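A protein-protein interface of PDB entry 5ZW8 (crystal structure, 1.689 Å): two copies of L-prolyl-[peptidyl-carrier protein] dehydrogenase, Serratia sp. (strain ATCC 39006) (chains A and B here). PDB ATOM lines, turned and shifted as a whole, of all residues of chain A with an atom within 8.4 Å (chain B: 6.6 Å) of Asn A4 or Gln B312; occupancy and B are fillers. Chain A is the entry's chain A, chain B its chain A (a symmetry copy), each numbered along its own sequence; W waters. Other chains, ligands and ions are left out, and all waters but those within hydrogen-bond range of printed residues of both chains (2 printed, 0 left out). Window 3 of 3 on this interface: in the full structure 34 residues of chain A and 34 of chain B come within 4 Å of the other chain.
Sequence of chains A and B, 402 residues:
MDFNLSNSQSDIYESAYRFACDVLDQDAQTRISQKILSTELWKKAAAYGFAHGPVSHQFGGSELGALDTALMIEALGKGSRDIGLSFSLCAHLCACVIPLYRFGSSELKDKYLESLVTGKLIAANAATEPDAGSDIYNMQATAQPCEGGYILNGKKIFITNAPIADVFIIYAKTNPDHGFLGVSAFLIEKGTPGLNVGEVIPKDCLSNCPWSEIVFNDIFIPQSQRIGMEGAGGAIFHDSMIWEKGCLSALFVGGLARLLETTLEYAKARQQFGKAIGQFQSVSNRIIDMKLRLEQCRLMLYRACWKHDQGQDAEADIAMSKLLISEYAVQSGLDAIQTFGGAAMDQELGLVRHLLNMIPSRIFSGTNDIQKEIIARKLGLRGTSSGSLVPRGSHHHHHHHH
Among the printed residues, pairs that only touch across the chains: Asp A2 with Trp B306, Phe A3 with Met B1, Phe A3 with Trp B306, Asn A4 with Trp B306, Asn A4 with Gln B312, Leu A67 with Met B1 and Tyr A302 with Met B1.
N of Met A1 lies within hydrogen-bond range of OD1 of Asp B2 (3.2 Å). The indole nitrogen of Trp B306 sits close to the backbone carbonyl oxygen of Met A1, 3.4 Å away. The side-chain carboxylate of Asp A2 sits at hydrogen-bond distance from the backbone NH of Met B1 (3.2 Å). The backbone carbonyl oxygen of Asp B2 sits at hydrogen-bond distance from the backbone NH of Asp A2. The backbone NH (N) of Met B1 lies within hydrogen-bond range of the backbone carbonyl oxygen (O) of Asn A4, at 2.5 Å.
OD1 of Asp A2 is in hydrogen-bond range of N of Asn A4. The backbone carbonyl oxygen of Lys B307 lies within hydrogen-bond range of the backbone NH of Gln B312, 3.0 Å away.
Asn A4 touches three residues of chain B. Printed residues of chain B within 4 Å of Leu A67: Met B1 (3.9 Å). Printed residues of chain B within 4 Å of Tyr A302: Met B1. Of chain A, only Asn A4 (3.7 Å) comes within 4 Å of Gln B312. Glu B315 touches none of the printed residues of chain A. The nearest printed residue of chain A that does not touch Met B1 is Leu A5 (4.2 Å).
Water W2 lies within hydrogen-bond range of N of Met B1 (2.8 Å) and OE1 of Gln A9 (3.0 Å). Water W1 bridges O of Met B1 and NE2 of Gln A9.
Hydrophobic or aromatic side chains of chain B that line the printed part of chain A: Met B1 and Trp B306. Printed residues of chain A that touch a printed residue of chain B: Met A1, Asp A2, Phe A3, Asn A4, Leu A67 and Tyr A302. Hydrophobic or aromatic side chains of chain A within 4 Å of the printed part of chain B: Met A1, Phe A3, Leu A67 and Tyr A302. Among the printed residues, no Asp or Glu carboxylate lies within 4 Å of a Lys or Arg side-chain nitrogen of the other chain.
Met A1 touches Asp B2, and with the chains exchanged Asp A2 touches Met B1. Asp A2 touches its own counterpart, Asp B2.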
ATOM      1  N   MET A   1       1.624 -11.509  12.731  1.00  0.00           N
ATOM      2  CA  MET A   1       1.592 -10.584  11.593  1.00  0.00           C
ATOM      3  C   MET A   1       1.150  -9.172  11.937  1.00  0.00           C
ATOM      4  O   MET A   1      -0.011  -8.980  12.278  1.00  0.00           O
ATOM      5  CB  MET A   1       0.669 -11.154  10.549  1.00  0.00           C
ATOM      6  CG  MET A   1       0.857 -10.550   9.182  1.00  0.00           C
ATOM      7  SD  MET A   1       1.474 -11.875   8.175  1.00  0.00           S
ATOM      8  CE  MET A   1       3.112 -11.475   8.296  1.00  0.00           C
ATOM      9  N   ASP A   2       2.055  -8.182  11.818  1.00  0.00           N
ATOM     10  CA  ASP A   2       1.844  -6.786  12.201  1.00  0.00           C
ATOM     11  C   ASP A   2       2.768  -5.973  11.315  1.00  0.00           C
ATOM     12  O   ASP A   2       3.936  -6.333  11.191  1.00  0.00           O
ATOM     13  CB  ASP A   2       2.211  -6.521  13.693  1.00  0.00           C
ATOM     14  CG  ASP A   2       1.981  -5.038  14.120  1.00  0.00           C
ATOM     15  OD1 ASP A   2       2.752  -4.125  13.751  1.00  0.00           O
ATOM     16  OD2 ASP A   2       0.982  -4.749  14.816  1.00  0.00           O
ATOM     17  N   PHE A   3       2.300  -4.881  10.728  1.00  0.00           N
ATOM     18  CA  PHE A   3       3.183  -4.113   9.851  1.00  0.00           C
ATOM     19  C   PHE A   3       3.416  -2.691  10.340  1.00  0.00           C
ATOM     20  O   PHE A   3       3.777  -1.816   9.537  1.00  0.00           O
ATOM     21  CB  PHE A   3       2.626  -4.103   8.428  1.00  0.00           C
ATOM     22  CG  PHE A   3       2.574  -5.477   7.827  1.00  0.00           C
ATOM     23  CD1 PHE A   3       3.681  -6.009   7.155  1.00  0.00           C
ATOM     24  CD2 PHE A   3       1.430  -6.262   7.948  1.00  0.00           C
ATOM     25  CE1 PHE A   3       3.647  -7.314   6.607  1.00  0.00           C
ATOM     26  CE2 PHE A   3       1.391  -7.554   7.413  1.00  0.00           C
ATOM     27  CZ  PHE A   3       2.498  -8.089   6.740  1.00  0.00           C
ATOM     28  N   ASN A   4       3.185  -2.446  11.621  1.00  0.00           N
ATOM     29  CA  ASN A   4       3.456  -1.167  12.270  1.00  0.00           C
ATOM     30  C   ASN A   4       4.813  -1.229  12.954  1.00  0.00           C
ATOM     31  O   ASN A   4       5.252  -2.278  13.435  1.00  0.00           O
ATOM     32  CB  ASN A   4       2.406  -0.820  13.346  1.00  0.00           C
ATOM     33  CG  ASN A   4       1.086  -0.238  12.789  1.00  0.00           C
ATOM     34  OD1 ASN A   4       1.037   0.445  11.733  1.00  0.00           O
ATOM     35  ND2 ASN A   4      -0.013  -0.503  13.543  1.00  0.00           N
ATOM     36  N   LEU A   5       5.485  -0.091  12.977  1.00  0.00           N
ATOM     37  CA  LEU A   5       6.678   0.036  13.788  1.00  0.00           C
ATOM     38  C   LEU A   5       6.255   0.268  15.248  1.00  0.00           C
ATOM     39  O   LEU A   5       5.270   0.968  15.514  1.00  0.00           O
ATOM     40  CB  LEU A   5       7.522   1.215  13.269  1.00  0.00           C
ATOM     41  CG  LEU A   5       8.187   1.133  11.881  1.00  0.00           C
ATOM     42  CD1 LEU A   5       9.097   2.343  11.694  1.00  0.00           C
ATOM     43  CD2 LEU A   5       8.940  -0.154  11.822  1.00  0.00           C
ATOM     44  N   SER A   6       7.012  -0.307  16.180  1.00  0.00           N
ATOM     45  CA  SER A   6       6.857   0.028  17.586  1.00  0.00           C
ATOM     46  C   SER A   6       7.232   1.496  17.828  1.00  0.00           C
ATOM     47  O   SER A   6       7.821   2.164  16.974  1.00  0.00           O
ATOM     48  CB  SER A   6       7.724  -0.883  18.426  1.00  0.00           C
ATOM     49  OG  SER A   6       9.099  -0.514  18.369  1.00  0.00           O
ATOM     50  N   ASN A   7       6.852   2.023  19.005  1.00  0.00           N
ATOM     51  CA  ASN A   7       7.258   3.394  19.309  1.00  0.00           C
ATOM     52  C   ASN A   7       8.775   3.502  19.365  1.00  0.00           C
ATOM     53  O   ASN A   7       9.358   4.489  18.894  1.00  0.00           O
ATOM     54  CB  ASN A   7       6.624   3.861  20.629  1.00  0.00           C
ATOM     55  CG  ASN A   7       5.124   3.973  20.527  1.00  0.00           C
ATOM     56  OD1 ASN A   7       4.591   4.459  19.518  1.00  0.00           O
ATOM     57  ND2 ASN A   7       4.419   3.501  21.561  1.00  0.00           N
ATOM     58  N   GLN A   9      10.939   1.762  17.686  1.00  0.00           N
ATOM     59  CA  GLN A   9      11.450   1.720  16.319  1.00  0.00           C
ATOM     60  C   GLN A   9      11.190   3.025  15.595  1.00  0.00           C
ATOM     61  O   GLN A   9      12.072   3.557  14.900  1.00  0.00           O
ATOM     62  CB  GLN A   9      10.791   0.551  15.595  1.00  0.00           C
ATOM     63  CG  GLN A   9      11.375  -0.820  15.973  1.00  0.00           C
ATOM     64  CD  GLN A   9      10.471  -1.968  15.494  1.00  0.00           C
ATOM     65  OE1 GLN A   9       9.247  -1.795  15.329  1.00  0.00           O
ATOM     66  NE2 GLN A   9      11.070  -3.127  15.246  1.00  0.00           N
ATOM     67  N   SER A  10       9.955   3.540  15.715  1.00  0.00           N
ATOM     68  CA  SER A  10       9.618   4.848  15.178  1.00  0.00           C
ATOM     69  C   SER A  10      10.569   5.942  15.682  1.00  0.00           C
ATOM     70  O   SER A  10      11.053   6.771  14.894  1.00  0.00           O
ATOM     71  CB  SER A  10       8.164   5.140  15.539  1.00  0.00           C
ATOM     72  OG  SER A  10       7.833   6.366  14.960  1.00  0.00           O
ATOM     73  N   LEU A  67      16.852  -5.257  12.649  1.00  0.00           N
ATOM     74  CA  LEU A  67      15.803  -4.399  12.121  1.00  0.00           C
ATOM     75  C   LEU A  67      15.998  -2.955  12.570  1.00  0.00           C
ATOM     76  O   LEU A  67      15.884  -2.027  11.749  1.00  0.00           O
ATOM     77  CB  LEU A  67      14.423  -4.949  12.498  1.00  0.00           C
ATOM     78  CG  LEU A  67      13.250  -4.131  12.016  1.00  0.00           C
ATOM     79  CD1 LEU A  67      13.270  -3.980  10.446  1.00  0.00           C
ATOM     80  CD2 LEU A  67      11.895  -4.724  12.493  1.00  0.00           C
ATOM     81  N   LEU A  71      16.560   0.249  10.171  1.00  0.00           N
ATOM     82  CA  LEU A  71      15.746   1.466  10.184  1.00  0.00           C
ATOM     83  C   LEU A  71      16.629   2.694  10.274  1.00  0.00           C
ATOM     84  O   LEU A  71      16.327   3.720   9.627  1.00  0.00           O
ATOM     85  CB  LEU A  71      14.723   1.431  11.344  1.00  0.00           C
ATOM     86  CG  LEU A  71      13.641   0.392  11.113  1.00  0.00           C
ATOM     87  CD1 LEU A  71      12.898   0.175  12.429  1.00  0.00           C
ATOM     88  CD2 LEU A  71      12.649   0.879  10.043  1.00  0.00           C
ATOM     89  N   LEU A 299       9.433  -4.281   2.387  1.00  0.00           N
ATOM     90  CA  LEU A 299       8.909  -5.408   3.164  1.00  0.00           C
ATOM     91  C   LEU A 299       9.881  -6.599   3.206  1.00  0.00           C
ATOM     92  O   LEU A 299      10.041  -7.276   4.261  1.00  0.00           O
ATOM     93  CB  LEU A 299       7.573  -5.840   2.570  1.00  0.00           C
ATOM     94  CG  LEU A 299       6.417  -4.867   2.871  1.00  0.00           C
ATOM     95  CD1 LEU A 299       5.179  -5.282   2.110  1.00  0.00           C
ATOM     96  CD2 LEU A 299       6.060  -4.821   4.369  1.00  0.00           C
ATOM     97  N   TYR A 302      12.670  -5.729   5.763  1.00  0.00           N
ATOM     98  CA  TYR A 302      12.190  -5.758   7.149  1.00  0.00           C
ATOM     99  C   TYR A 302      11.988  -7.189   7.603  1.00  0.00           C
ATOM    100  O   TYR A 302      12.381  -7.562   8.727  1.00  0.00           O
ATOM    101  CB  TYR A 302      10.860  -5.014   7.273  1.00  0.00           C
ATOM    102  CG  TYR A 302      10.961  -3.510   7.143  1.00  0.00           C
ATOM    103  CD1 TYR A 302      12.191  -2.877   7.036  1.00  0.00           C
ATOM    104  CD2 TYR A 302       9.822  -2.736   7.252  1.00  0.00           C
ATOM    105  CE1 TYR A 302      12.285  -1.469   6.950  1.00  0.00           C
ATOM    106  CE2 TYR A 302       9.890  -1.353   7.193  1.00  0.00           C
ATOM    107  CZ  TYR A 302      11.121  -0.723   7.052  1.00  0.00           C
ATOM    108  OH  TYR A 302      11.132   0.662   6.985  1.00  0.00           O
ATOM    109  N   MET B   1       5.891  -4.641  14.051  1.00  0.00           N
ATOM    110  CA  MET B   1       6.461  -5.476  12.989  1.00  0.00           C
ATOM    111  C   MET B   1       6.721  -6.919  13.389  1.00  0.00           C
ATOM    112  O   MET B   1       7.597  -7.158  14.211  1.00  0.00           O
ATOM    113  CB  MET B   1       7.750  -4.847  12.533  1.00  0.00           C
ATOM    114  CG  MET B   1       8.224  -5.341  11.192  1.00  0.00           C
ATOM    115  SD  MET B   1       8.116  -3.932  10.118  1.00  0.00           S
ATOM    116  CE  MET B   1       6.613  -4.309   9.441  1.00  0.00           C
ATOM    117  N   ASP B   2       5.991  -7.880  12.792  1.00  0.00           N
ATOM    118  CA  ASP B   2       6.027  -9.305  13.121  1.00  0.00           C
ATOM    119  C   ASP B   2       5.630 -10.030  11.851  1.00  0.00           C
ATOM    120  O   ASP B   2       4.645  -9.641  11.231  1.00  0.00           O
ATOM    121  CB  ASP B   2       5.019  -9.675  14.252  1.00  0.00           C
ATOM    122  CG  ASP B   2       5.054 -11.191  14.623  1.00  0.00           C
ATOM    123  OD1 ASP B   2       4.557 -12.058  13.872  1.00  0.00           O
ATOM    124  OD2 ASP B   2       5.626 -11.550  15.676  1.00  0.00           O
ATOM    125  N   ALA B 304      -1.760  -5.569   2.878  1.00  0.00           N
ATOM    126  CA  ALA B 304      -2.972  -4.894   2.465  1.00  0.00           C
ATOM    127  C   ALA B 304      -4.160  -5.349   3.329  1.00  0.00           C
ATOM    128  O   ALA B 304      -4.928  -4.515   3.847  1.00  0.00           O
ATOM    129  CB  ALA B 304      -3.268  -5.156   0.990  1.00  0.00           C
ATOM    130  N   TRP B 306      -4.095  -6.871   6.337  1.00  0.00           N
ATOM    131  CA  TRP B 306      -3.895  -6.483   7.724  1.00  0.00           C
ATOM    132  C   TRP B 306      -4.216  -5.006   7.927  1.00  0.00           C
ATOM    133  O   TRP B 306      -4.875  -4.648   8.907  1.00  0.00           O
ATOM    134  CB  TRP B 306      -2.462  -6.790   8.133  1.00  0.00           C
ATOM    135  CG  TRP B 306      -2.080  -6.267   9.507  1.00  0.00           C
ATOM    136  CD1 TRP B 306      -2.182  -6.934  10.726  1.00  0.00           C
ATOM    137  CD2 TRP B 306      -1.549  -4.965   9.812  1.00  0.00           C
ATOM    138  NE1 TRP B 306      -1.720  -6.121  11.741  1.00  0.00           N
ATOM    139  CE2 TRP B 306      -1.340  -4.910  11.205  1.00  0.00           C
ATOM    140  CE3 TRP B 306      -1.210  -3.854   9.035  1.00  0.00           C
ATOM    141  CZ2 TRP B 306      -0.793  -3.789  11.812  1.00  0.00           C
ATOM    142  CZ3 TRP B 306      -0.702  -2.746   9.649  1.00  0.00           C
ATOM    143  CH2 TRP B 306      -0.488  -2.719  11.008  1.00  0.00           C
ATOM    144  N   LYS B 307      -3.811  -4.136   6.984  1.00  0.00           N
ATOM    145  CA  LYS B 307      -4.163  -2.721   7.106  1.00  0.00           C
ATOM    146  C   LYS B 307      -5.668  -2.552   7.141  1.00  0.00           C
ATOM    147  O   LYS B 307      -6.195  -1.826   7.979  1.00  0.00           O
ATOM    148  CB  LYS B 307      -3.564  -1.879   5.966  1.00  0.00           C
ATOM    149  CG  LYS B 307      -2.057  -1.716   6.112  1.00  0.00           C
ATOM    150  CD  LYS B 307      -1.384  -0.922   4.975  1.00  0.00           C
ATOM    151  CE  LYS B 307      -1.841   0.515   4.924  1.00  0.00           C
ATOM    152  NZ  LYS B 307      -1.062   1.268   3.882  1.00  0.00           N
ATOM    153  N   HIS B 308      -6.377  -3.230   6.245  1.00  0.00           N
ATOM    154  CA  HIS B 308      -7.835  -3.219   6.305  1.00  0.00           C
ATOM    155  C   HIS B 308      -8.353  -3.674   7.661  1.00  0.00           C
ATOM    156  O   HIS B 308      -9.226  -3.021   8.279  1.00  0.00           O
ATOM    157  CB  HIS B 308      -8.404  -4.104   5.208  1.00  0.00           C
ATOM    158  CG  HIS B 308      -9.886  -4.216   5.299  1.00  0.00           C
ATOM    159  ND1 HIS B 308     -10.731  -3.334   4.665  1.00  0.00           N
ATOM    160  CD2 HIS B 308     -10.673  -5.046   6.026  1.00  0.00           C
ATOM    161  CE1 HIS B 308     -11.984  -3.654   4.945  1.00  0.00           C
ATOM    162  NE2 HIS B 308     -11.977  -4.665   5.797  1.00  0.00           N
ATOM    163  N   ASP B 309      -7.824  -4.776   8.170  1.00  0.00           N
ATOM    164  CA  ASP B 309      -8.277  -5.249   9.478  1.00  0.00           C
ATOM    165  C   ASP B 309      -7.990  -4.227  10.580  1.00  0.00           C
ATOM    166  O   ASP B 309      -8.673  -4.227  11.613  1.00  0.00           O
ATOM    167  CB  ASP B 309      -7.636  -6.569   9.840  1.00  0.00           C
ATOM    168  CG  ASP B 309      -8.149  -7.693   8.969  1.00  0.00           C
ATOM    169  OD1 ASP B 309      -9.231  -7.473   8.360  1.00  0.00           O
ATOM    170  OD2 ASP B 309      -7.490  -8.760   8.934  1.00  0.00           O
ATOM    171  N   GLN B 310      -6.970  -3.390  10.401  1.00  0.00           N
ATOM    172  CA  GLN B 310      -6.628  -2.379  11.383  1.00  0.00           C
ATOM    173  C   GLN B 310      -7.479  -1.132  11.265  1.00  0.00           C
ATOM    174  O   GLN B 310      -7.326  -0.212  12.070  1.00  0.00           O
ATOM    175  CB  GLN B 310      -5.150  -2.007  11.235  1.00  0.00           C
ATOM    176  CG  GLN B 310      -4.271  -3.103  11.665  1.00  0.00           C
ATOM    177  CD  GLN B 310      -4.246  -3.225  13.142  1.00  0.00           C
ATOM    178  OE1 GLN B 310      -4.048  -2.230  13.841  1.00  0.00           O
ATOM    179  NE2 GLN B 310      -4.401  -4.435  13.645  1.00  0.00           N
ATOM    180  N   GLY B 311      -8.327  -1.038  10.278  1.00  0.00           N
ATOM    181  CA  GLY B 311      -9.055   0.168  10.049  1.00  0.00           C
ATOM    182  C   GLY B 311      -8.346   1.175   9.180  1.00  0.00           C
ATOM    183  O   GLY B 311      -8.909   2.244   8.932  1.00  0.00           O
ATOM    184  N   GLN B 312      -7.123   0.886   8.723  1.00  0.00           N
ATOM    185  CA  GLN B 312      -6.434   1.832   7.858  1.00  0.00           C
ATOM    186  C   GLN B 312      -6.932   1.726   6.416  1.00  0.00           C
ATOM    187  O   GLN B 312      -7.571   0.750   6.018  1.00  0.00           O
ATOM    188  CB  GLN B 312      -4.931   1.625   7.926  1.00  0.00           C
ATOM    189  CG  GLN B 312      -4.432   1.572   9.332  1.00  0.00           C
ATOM    190  CD  GLN B 312      -2.958   1.211   9.416  1.00  0.00           C
ATOM    191  OE1 GLN B 312      -2.245   1.302   8.429  1.00  0.00           O
ATOM    192  NE2 GLN B 312      -2.495   0.826  10.607  1.00  0.00           N
ATOM    193  N   ASP B 313      -6.661   2.775   5.649  1.00  0.00           N
ATOM    194  CA  ASP B 313      -7.028   2.848   4.233  1.00  0.00           C
ATOM    195  C   ASP B 313      -6.179   1.873   3.420  1.00  0.00           C
ATOM    196  O   ASP B 313      -4.957   2.036   3.338  1.00  0.00           O
ATOM    197  CB  ASP B 313      -6.787   4.261   3.706  1.00  0.00           C
ATOM    198  CG  ASP B 313      -7.515   5.324   4.496  1.00  0.00           C
ATOM    199  OD1 ASP B 313      -8.363   4.982   5.369  1.00  0.00           O
ATOM    200  OD2 ASP B 313      -7.219   6.517   4.233  1.00  0.00           O
ATOM    201  N   ALA B 314      -6.799   0.856   2.838  1.00  0.00           N
ATOM    202  CA  ALA B 314      -6.019  -0.227   2.234  1.00  0.00           C
ATOM    203  C   ALA B 314      -6.304  -0.360   0.753  1.00  0.00           C
ATOM    204  O   ALA B 314      -5.809  -1.310   0.133  1.00  0.00           O
ATOM    205  CB  ALA B 314      -6.275  -1.570   2.915  1.00  0.00           C
ATOM    206  N   GLU B 315      -7.057   0.573   0.165  1.00  0.00           N
ATOM    207  CA  GLU B 315      -7.478   0.384  -1.212  1.00  0.00           C
ATOM    208  C   GLU B 315      -6.296   0.429  -2.181  1.00  0.00           C
ATOM    209  O   GLU B 315      -6.224  -0.385  -3.114  1.00  0.00           O
ATOM    210  CB  GLU B 315      -8.508   1.431  -1.608  1.00  0.00           C
ATOM    211  CG  GLU B 315      -8.923   1.279  -3.077  1.00  0.00           C
ATOM    212  CD  GLU B 315     -10.025   2.237  -3.475  1.00  0.00           C
ATOM    213  OE1 GLU B 315     -10.429   3.038  -2.586  1.00  0.00           O
ATOM    214  OE2 GLU B 315     -10.475   2.178  -4.650  1.00  0.00           O
HETATM  215  O   HOH W   1       9.889  -5.900  15.526  1.00  0.00           O
HETATM  216  O   HOH W   2       7.553  -4.064  16.198  1.00  0.00           O
